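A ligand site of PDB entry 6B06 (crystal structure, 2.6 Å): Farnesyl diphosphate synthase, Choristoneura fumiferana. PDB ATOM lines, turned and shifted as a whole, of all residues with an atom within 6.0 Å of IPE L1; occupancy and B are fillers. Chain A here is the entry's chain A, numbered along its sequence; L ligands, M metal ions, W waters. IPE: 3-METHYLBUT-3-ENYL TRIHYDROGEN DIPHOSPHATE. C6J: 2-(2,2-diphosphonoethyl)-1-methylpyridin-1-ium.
The side-chain amide nitrogen (NE2) of Gln 84 sits at hydrogen-bond distance from an oxygen (O3B) of IPE L1. The backbone NH (N) of Lys 45 lies within hydrogen-bond range of an oxygen (O1B) of IPE L1, 3.1 Å away. An oxygen (O1B) of IPE L1 is in salt-bridge range of the side-chain amino group of Lys 45 (3.2 Å). NZ of Lys 245 lies within salt-bridge range of OAO of C6J L2 (3.3 Å). The side-chain amino group of Lys 188 is in salt-bridge range of an oxygen (OAM) of C6J L2. The guanidinium group (NH2) of Arg 48 lies within salt-bridge range of an oxygen (O2A) of IPE L1 (2.6 Å). NE of Arg 101 lies within salt-bridge range of O2B of IPE L1 (3.0 Å). OAO of C6J L2 lies within salt-bridge range of NH1 of Arg 100 (2.8 Å).
The guanidinium group (NH1) of Arg 48 lies within hydrogen-bond range of the side-chain amide oxygen (OE1) of Gln 84 (3.3 Å). The side-chain amino group (NZ) of Lys 45 is in salt-bridge range of the chain-end carboxylate (OXT) of His 341 (3.1 Å). The side-chain hydroxyl (OH) of Tyr 192 lies within hydrogen-bond range of the guanidinium group (NH1) of Arg 48 (3.1 Å). OE1 of Gln 84 sits at hydrogen-bond distance from OH of Tyr 192, at 2.8 Å. The side-chain carboxylate (OD1) of Asp 231 lies within salt-bridge range of the side-chain amino group (NZ) of Lys 245 (2.7 Å). The side-chain amide oxygen of Gln 228 sits close to the side-chain carboxylate of Asp 231, 3.4 Å away. OG1 of Thr 193 lies within hydrogen-bond range of NH1 of Arg 48 (3.1 Å). The backbone carbonyl oxygen of Phe 227 sits close to the guanidinium group of Arg 339.
Residues that only touch IPE L1: Gly 44, Arg 100, Tyr 192, Phe 227 and Asp 231. Of the 21 residues printed, 9 come within 4 Å of IPE L1.
Water W2 lies within hydrogen-bond range of an oxygen (O1B) of IPE L1, the backbone NH of Ala 47 and the backbone NH of Lys 46. Water W1 lies within hydrogen-bond range of the side-chain carboxylate of Glu 81 (2.7 Å), the backbone NH of Lys 46 (3.0 Å) and an oxygen (O3B) of IPE L1 (3.3 Å).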
ATOM      1  N   GLY A  43     -29.964 -20.389  24.137  1.00  0.00           N
ATOM      2  CA  GLY A  43     -30.168 -19.323  23.116  1.00  0.00           C
ATOM      3  C   GLY A  43     -29.746 -19.961  21.814  1.00  0.00           C
ATOM      4  O   GLY A  43     -29.862 -21.192  21.662  1.00  0.00           O
ATOM      5  N   GLY A  44     -29.244 -19.165  20.881  1.00  0.00           N
ATOM      6  CA  GLY A  44     -28.509 -19.748  19.723  1.00  0.00           C
ATOM      7  C   GLY A  44     -29.330 -20.501  18.685  1.00  0.00           C
ATOM      8  O   GLY A  44     -30.356 -21.106  18.968  1.00  0.00           O
ATOM      9  N   LYS A  45     -28.879 -20.466  17.443  1.00  0.00           N
ATOM     10  CA  LYS A  45     -29.702 -20.998  16.351  1.00  0.00           C
ATOM     11  C   LYS A  45     -29.460 -22.458  16.151  1.00  0.00           C
ATOM     12  O   LYS A  45     -30.165 -23.085  15.383  1.00  0.00           O
ATOM     13  CB  LYS A  45     -29.431 -20.230  15.040  1.00  0.00           C
ATOM     14  CG  LYS A  45     -29.644 -18.717  15.135  1.00  0.00           C
ATOM     15  CD  LYS A  45     -29.233 -17.984  13.866  1.00  0.00           C
ATOM     16  CE  LYS A  45     -27.713 -17.864  13.720  1.00  0.00           C
ATOM     17  NZ  LYS A  45     -27.175 -16.713  14.504  1.00  0.00           N
ATOM     18  N   LYS A  46     -28.444 -23.006  16.830  1.00  0.00           N
ATOM     19  CA  LYS A  46     -28.068 -24.403  16.691  1.00  0.00           C
ATOM     20  C   LYS A  46     -27.760 -24.828  15.238  1.00  0.00           C
ATOM     21  O   LYS A  46     -27.849 -25.999  14.878  1.00  0.00           O
ATOM     22  CB  LYS A  46     -29.099 -25.333  17.377  1.00  0.00           C
ATOM     23  CG  LYS A  46     -28.853 -25.597  18.875  1.00  0.00           C
ATOM     24  CD  LYS A  46     -29.741 -24.798  19.821  1.00  0.00           C
ATOM     25  CE  LYS A  46     -29.295 -24.950  21.278  1.00  0.00           C
ATOM     26  NZ  LYS A  46     -29.949 -23.918  22.146  1.00  0.00           N
ATOM     27  N   ALA A  47     -27.329 -23.876  14.429  1.00  0.00           N
ATOM     28  CA  ALA A  47     -27.063 -24.078  13.026  1.00  0.00           C
ATOM     29  C   ALA A  47     -26.033 -25.142  12.711  1.00  0.00           C
ATOM     30  O   ALA A  47     -26.284 -25.973  11.863  1.00  0.00           O
ATOM     31  CB  ALA A  47     -26.639 -22.758  12.394  1.00  0.00           C
ATOM     32  N   ARG A  48     -24.891 -25.139  13.401  1.00  0.00           N
ATOM     33  CA  ARG A  48     -23.846 -26.143  13.120  1.00  0.00           C
ATOM     34  C   ARG A  48     -24.307 -27.557  13.435  1.00  0.00           C
ATOM     35  O   ARG A  48     -23.940 -28.513  12.752  1.00  0.00           O
ATOM     36  CB  ARG A  48     -22.555 -25.962  13.929  1.00  0.00           C
ATOM     37  CG  ARG A  48     -21.991 -24.594  14.153  1.00  0.00           C
ATOM     38  CD  ARG A  48     -21.886 -23.803  12.889  1.00  0.00           C
ATOM     39  NE  ARG A  48     -22.272 -22.418  13.112  1.00  0.00           N
ATOM     40  CZ  ARG A  48     -21.555 -21.517  13.787  1.00  0.00           C
ATOM     41  NH1 ARG A  48     -20.401 -21.829  14.338  1.00  0.00           N
ATOM     42  NH2 ARG A  48     -22.003 -20.275  13.908  1.00  0.00           N
ATOM     43  N   GLU A  81     -21.575 -28.275  18.608  1.00  0.00           N
ATOM     44  CA  GLU A  81     -22.122 -27.119  19.295  1.00  0.00           C
ATOM     45  C   GLU A  81     -21.361 -26.829  20.579  1.00  0.00           C
ATOM     46  O   GLU A  81     -21.337 -25.691  21.026  1.00  0.00           O
ATOM     47  CB  GLU A  81     -23.616 -27.261  19.559  1.00  0.00           C
ATOM     48  CG  GLU A  81     -24.513 -26.863  18.368  1.00  0.00           C
ATOM     49  CD  GLU A  81     -24.666 -25.362  18.131  1.00  0.00           C
ATOM     50  OE1 GLU A  81     -24.893 -24.601  19.112  1.00  0.00           O
ATOM     51  OE2 GLU A  81     -24.554 -24.947  16.944  1.00  0.00           O
ATOM     52  N   GLN A  84     -18.370 -24.979  19.661  1.00  0.00           N
ATOM     53  CA  GLN A  84     -18.790 -23.627  19.456  1.00  0.00           C
ATOM     54  C   GLN A  84     -18.889 -22.897  20.759  1.00  0.00           C
ATOM     55  O   GLN A  84     -18.497 -21.734  20.818  1.00  0.00           O
ATOM     56  CB  GLN A  84     -20.139 -23.620  18.708  1.00  0.00           C
ATOM     57  CG  GLN A  84     -21.065 -22.431  18.888  1.00  0.00           C
ATOM     58  CD  GLN A  84     -20.890 -21.391  17.801  1.00  0.00           C
ATOM     59  OE1 GLN A  84     -19.764 -21.022  17.463  1.00  0.00           O
ATOM     60  NE2 GLN A  84     -21.994 -20.924  17.260  1.00  0.00           N
ATOM     61  N   VAL A  88     -16.485 -19.601  21.524  1.00  0.00           N
ATOM     62  CA  VAL A  88     -17.026 -18.247  21.857  1.00  0.00           C
ATOM     63  C   VAL A  88     -16.855 -17.888  23.315  1.00  0.00           C
ATOM     64  O   VAL A  88     -16.839 -16.737  23.624  1.00  0.00           O
ATOM     65  CB  VAL A  88     -18.507 -17.950  21.481  1.00  0.00           C
ATOM     66  CG1 VAL A  88     -18.830 -18.430  20.070  1.00  0.00           C
ATOM     67  CG2 VAL A  88     -19.482 -18.472  22.494  1.00  0.00           C
ATOM     68  N   ARG A 100     -23.787 -12.368  25.317  1.00  0.00           N
ATOM     69  CA  ARG A 100     -23.914 -13.268  24.195  1.00  0.00           C
ATOM     70  C   ARG A 100     -25.188 -14.104  24.293  1.00  0.00           C
ATOM     71  O   ARG A 100     -25.481 -14.665  25.350  1.00  0.00           O
ATOM     72  CB  ARG A 100     -22.707 -14.211  24.116  1.00  0.00           C
ATOM     73  CG  ARG A 100     -22.969 -15.342  23.114  1.00  0.00           C
ATOM     74  CD  ARG A 100     -21.742 -16.031  22.618  1.00  0.00           C
ATOM     75  NE  ARG A 100     -20.698 -15.084  22.263  1.00  0.00           N
ATOM     76  CZ  ARG A 100     -20.317 -14.749  21.023  1.00  0.00           C
ATOM     77  NH1 ARG A 100     -20.863 -15.300  19.944  1.00  0.00           N
ATOM     78  NH2 ARG A 100     -19.332 -13.859  20.887  1.00  0.00           N
ATOM     79  N   ARG A 101     -25.904 -14.238  23.170  1.00  0.00           N
ATOM     80  CA  ARG A 101     -27.181 -14.988  23.130  1.00  0.00           C
ATOM     81  C   ARG A 101     -28.205 -14.491  24.187  1.00  0.00           C
ATOM     82  O   ARG A 101     -28.972 -15.283  24.775  1.00  0.00           O
ATOM     83  CB  ARG A 101     -26.938 -16.503  23.292  1.00  0.00           C
ATOM     84  CG  ARG A 101     -26.137 -17.201  22.191  1.00  0.00           C
ATOM     85  CD  ARG A 101     -25.468 -18.470  22.726  1.00  0.00           C
ATOM     86  NE  ARG A 101     -24.872 -19.321  21.681  1.00  0.00           N
ATOM     87  CZ  ARG A 101     -24.051 -20.361  21.890  1.00  0.00           C
ATOM     88  NH1 ARG A 101     -23.687 -20.723  23.123  1.00  0.00           N
ATOM     89  NH2 ARG A 101     -23.585 -21.057  20.862  1.00  0.00           N
ATOM     90  N   LYS A 188     -10.776 -19.100  10.779  1.00  0.00           N
ATOM     91  CA  LYS A 188     -11.521 -18.934  12.049  1.00  0.00           C
ATOM     92  C   LYS A 188     -13.010 -19.273  12.038  1.00  0.00           C
ATOM     93  O   LYS A 188     -13.608 -19.444  13.086  1.00  0.00           O
ATOM     94  CB  LYS A 188     -11.346 -17.545  12.661  1.00  0.00           C
ATOM     95  CG  LYS A 188     -12.227 -16.459  12.131  1.00  0.00           C
ATOM     96  CD  LYS A 188     -12.331 -15.289  13.068  1.00  0.00           C
ATOM     97  CE  LYS A 188     -12.964 -14.153  12.264  1.00  0.00           C
ATOM     98  NZ  LYS A 188     -13.772 -13.237  13.098  1.00  0.00           N
ATOM     99  N   THR A 189     -13.609 -19.316  10.863  1.00  0.00           N
ATOM    100  CA  THR A 189     -15.068 -19.484  10.742  1.00  0.00           C
ATOM    101  C   THR A 189     -15.411 -20.574   9.761  1.00  0.00           C
ATOM    102  O   THR A 189     -16.073 -21.520  10.147  1.00  0.00           O
ATOM    103  CB  THR A 189     -15.701 -18.186  10.271  1.00  0.00           C
ATOM    104  OG1 THR A 189     -15.295 -17.162  11.177  1.00  0.00           O
ATOM    105  CG2 THR A 189     -17.223 -18.289  10.224  1.00  0.00           C
ATOM    106  N   TYR A 192     -14.769 -24.731  10.719  1.00  0.00           N
ATOM    107  CA  TYR A 192     -15.515 -25.400  11.773  1.00  0.00           C
ATOM    108  C   TYR A 192     -17.004 -25.218  11.634  1.00  0.00           C
ATOM    109  O   TYR A 192     -17.749 -25.995  12.215  1.00  0.00           O
ATOM    110  CB  TYR A 192     -15.071 -24.990  13.179  1.00  0.00           C
ATOM    111  CG  TYR A 192     -15.828 -23.843  13.786  1.00  0.00           C
ATOM    112  CD1 TYR A 192     -15.417 -22.524  13.560  1.00  0.00           C
ATOM    113  CD2 TYR A 192     -16.907 -24.046  14.619  1.00  0.00           C
ATOM    114  CE1 TYR A 192     -16.105 -21.456  14.113  1.00  0.00           C
ATOM    115  CE2 TYR A 192     -17.590 -22.990  15.192  1.00  0.00           C
ATOM    116  CZ  TYR A 192     -17.178 -21.687  14.935  1.00  0.00           C
ATOM    117  OH  TYR A 192     -17.826 -20.617  15.482  1.00  0.00           O
ATOM    118  N   THR A 193     -17.424 -24.195  10.891  1.00  0.00           N
ATOM    119  CA  THR A 193     -18.836 -23.847  10.731  1.00  0.00           C
ATOM    120  C   THR A 193     -19.536 -24.596   9.616  1.00  0.00           C
ATOM    121  O   THR A 193     -20.735 -24.774   9.693  1.00  0.00           O
ATOM    122  CB  THR A 193     -18.970 -22.314  10.563  1.00  0.00           C
ATOM    123  OG1 THR A 193     -18.553 -21.706  11.791  1.00  0.00           O
ATOM    124  CG2 THR A 193     -20.363 -21.852  10.252  1.00  0.00           C
ATOM    125  N   PHE A 227     -20.967 -16.359   5.170  1.00  0.00           N
ATOM    126  CA  PHE A 227     -21.543 -16.357   6.506  1.00  0.00           C
ATOM    127  C   PHE A 227     -20.917 -15.311   7.408  1.00  0.00           C
ATOM    128  O   PHE A 227     -21.629 -14.606   8.115  1.00  0.00           O
ATOM    129  CB  PHE A 227     -21.404 -17.748   7.175  1.00  0.00           C
ATOM    130  CG  PHE A 227     -21.961 -17.805   8.563  1.00  0.00           C
ATOM    131  CD1 PHE A 227     -23.302 -17.942   8.776  1.00  0.00           C
ATOM    132  CD2 PHE A 227     -21.128 -17.667   9.655  1.00  0.00           C
ATOM    133  CE1 PHE A 227     -23.827 -17.968  10.050  1.00  0.00           C
ATOM    134  CE2 PHE A 227     -21.657 -17.689  10.953  1.00  0.00           C
ATOM    135  CZ  PHE A 227     -23.020 -17.857  11.143  1.00  0.00           C
ATOM    136  N   GLN A 228     -19.593 -15.231   7.362  1.00  0.00           N
ATOM    137  CA  GLN A 228     -18.810 -14.340   8.201  1.00  0.00           C
ATOM    138  C   GLN A 228     -18.887 -12.855   7.753  1.00  0.00           C
ATOM    139  O   GLN A 228     -18.778 -11.962   8.582  1.00  0.00           O
ATOM    140  CB  GLN A 228     -17.352 -14.843   8.274  1.00  0.00           C
ATOM    141  CG  GLN A 228     -16.407 -14.044   9.162  1.00  0.00           C
ATOM    142  CD  GLN A 228     -16.812 -14.006  10.621  1.00  0.00           C
ATOM    143  OE1 GLN A 228     -16.969 -12.945  11.215  1.00  0.00           O
ATOM    144  NE2 GLN A 228     -17.002 -15.165  11.189  1.00  0.00           N
ATOM    145  N   ASP A 231     -21.981 -11.906   9.517  1.00  0.00           N
ATOM    146  CA  ASP A 231     -21.659 -11.673  10.922  1.00  0.00           C
ATOM    147  C   ASP A 231     -21.052 -10.304  11.094  1.00  0.00           C
ATOM    148  O   ASP A 231     -21.393  -9.600  12.037  1.00  0.00           O
ATOM    149  CB  ASP A 231     -20.693 -12.696  11.493  1.00  0.00           C
ATOM    150  CG  ASP A 231     -20.484 -12.508  13.029  1.00  0.00           C
ATOM    151  OD1 ASP A 231     -21.532 -12.638  13.720  1.00  0.00           O
ATOM    152  OD2 ASP A 231     -19.307 -12.223  13.544  1.00  0.00           O
ATOM    153  N   LYS A 245     -26.119  -9.980  21.307  1.00  0.00           N
ATOM    154  CA  LYS A 245     -24.749  -9.536  21.599  1.00  0.00           C
ATOM    155  C   LYS A 245     -24.545  -8.059  21.229  1.00  0.00           C
ATOM    156  O   LYS A 245     -25.215  -7.526  20.347  1.00  0.00           O
ATOM    157  CB  LYS A 245     -23.712 -10.428  20.884  1.00  0.00           C
ATOM    158  CG  LYS A 245     -24.013 -10.753  19.411  1.00  0.00           C
ATOM    159  CD  LYS A 245     -22.831 -11.414  18.662  1.00  0.00           C
ATOM    160  CE  LYS A 245     -22.977 -11.295  17.128  1.00  0.00           C
ATOM    161  NZ  LYS A 245     -22.324 -12.389  16.325  1.00  0.00           N
ATOM    162  N   ARG A 339     -30.335 -13.277   6.313  1.00  0.00           N
ATOM    163  CA  ARG A 339     -30.470 -13.351   7.763  1.00  0.00           C
ATOM    164  C   ARG A 339     -30.126 -12.044   8.444  1.00  0.00           C
ATOM    165  O   ARG A 339     -29.436 -11.205   7.868  1.00  0.00           O
ATOM    166  CB  ARG A 339     -29.648 -14.503   8.333  1.00  0.00           C
ATOM    167  CG  ARG A 339     -28.179 -14.230   8.647  1.00  0.00           C
ATOM    168  CD  ARG A 339     -27.437 -15.559   8.844  1.00  0.00           C
ATOM    169  NE  ARG A 339     -25.982 -15.424   8.995  1.00  0.00           N
ATOM    170  CZ  ARG A 339     -25.336 -15.007  10.089  1.00  0.00           C
ATOM    171  NH1 ARG A 339     -26.000 -14.662  11.181  1.00  0.00           N
ATOM    172  NH2 ARG A 339     -24.018 -14.931  10.098  1.00  0.00           N
ATOM    173  N   HIS A 341     -29.654 -11.998  12.259  1.00  0.00           N
ATOM    174  CA  HIS A 341     -29.144 -12.231  13.612  1.00  0.00           C
ATOM    175  C   HIS A 341     -28.223 -13.449  13.663  1.00  0.00           C
ATOM    176  O   HIS A 341     -27.341 -13.522  14.503  1.00  0.00           O
ATOM    177  CB  HIS A 341     -30.309 -12.359  14.631  1.00  0.00           C
ATOM    178  CG  HIS A 341     -31.076 -13.635  14.529  1.00  0.00           C
ATOM    179  ND1 HIS A 341     -32.122 -13.812  13.647  1.00  0.00           N
ATOM    180  CD2 HIS A 341     -30.938 -14.805  15.204  1.00  0.00           C
ATOM    181  CE1 HIS A 341     -32.598 -15.040  13.770  1.00  0.00           C
ATOM    182  NE2 HIS A 341     -31.898 -15.661  14.707  1.00  0.00           N
ATOM    183  OXT HIS A 341     -28.323 -14.384  12.889  1.00  0.00           O
HETATM  184  C1  IPE L   1     -21.238 -17.028  16.402  1.00  0.00           C
HETATM  185  O1  IPE L   1     -21.932 -17.843  15.447  1.00  0.00           O
HETATM  186  C2  IPE L   1     -19.763 -17.019  16.104  1.00  0.00           C
HETATM  187  C3  IPE L   1     -19.525 -16.788  14.639  1.00  0.00           C
HETATM  188  C4  IPE L   1     -18.768 -17.619  13.929  1.00  0.00           C
HETATM  189  C5  IPE L   1     -20.163 -15.599  14.010  1.00  0.00           C
HETATM  190  PA  IPE L   1     -23.549 -17.837  15.457  1.00  0.00           P
HETATM  191  O1A IPE L   1     -23.894 -16.388  15.163  1.00  0.00           O
HETATM  192  O2A IPE L   1     -24.109 -19.023  14.671  1.00  0.00           O
HETATM  193  O3A IPE L   1     -23.906 -18.089  17.027  1.00  0.00           O
HETATM  194  PB  IPE L   1     -25.117 -18.953  17.692  1.00  0.00           P
HETATM  195  O1B IPE L   1     -26.286 -18.900  16.722  1.00  0.00           O
HETATM  196  O2B IPE L   1     -25.356 -18.102  18.932  1.00  0.00           O
HETATM  197  O3B IPE L   1     -24.586 -20.382  17.896  1.00  0.00           O
HETATM  198  OAL C6J L   2     -16.428 -11.849  15.080  1.00  0.00           O
HETATM  199  PAK C6J L   2     -16.045 -13.004  16.018  1.00  0.00           P
HETATM  200  OAN C6J L   2     -15.750 -12.352  17.531  1.00  0.00           O
HETATM  201  OAM C6J L   2     -14.941 -13.672  15.421  1.00  0.00           O
HETATM  202  CAH C6J L   2     -17.482 -14.048  16.365  1.00  0.00           C
HETATM  203  PAI C6J L   2     -18.648 -13.009  17.305  1.00  0.00           P
HETATM  204  OAO C6J L   2     -19.857 -14.027  17.712  1.00  0.00           O
HETATM  205  OAQ C6J L   2     -17.852 -12.607  18.655  1.00  0.00           O
HETATM  206  OAP C6J L   2     -19.125 -11.827  16.540  1.00  0.00           O
HETATM  207  CAG C6J L   2     -17.046 -15.166  17.271  1.00  0.00           C
HETATM  208  CAE C6J L   2     -16.193 -16.156  16.681  1.00  0.00           C
HETATM  209  CAD C6J L   2     -15.530 -16.898  17.642  1.00  0.00           C
HETATM  210  CAC C6J L   2     -14.660 -17.919  17.351  1.00  0.00           C
HETATM  211  CAB C6J L   2     -14.416 -18.250  16.056  1.00  0.00           C
HETATM  212  CAA C6J L   2     -15.059 -17.542  15.088  1.00  0.00           C
HETATM  213  NAF C6J L   2     -15.944 -16.533  15.391  1.00  0.00           N
HETATM  214  CAJ C6J L   2     -16.418 -15.942  14.111  1.00  0.00           C
HETATM  215 MG    MG M   1     -18.293 -10.324  15.280  1.00  0.00          MG
HETATM  216  O   HOH W   1     -26.616 -22.578  19.233  1.00  0.00           O
HETATM  217  O   HOH W   2     -26.203 -21.207  15.129  1.00  0.00           O
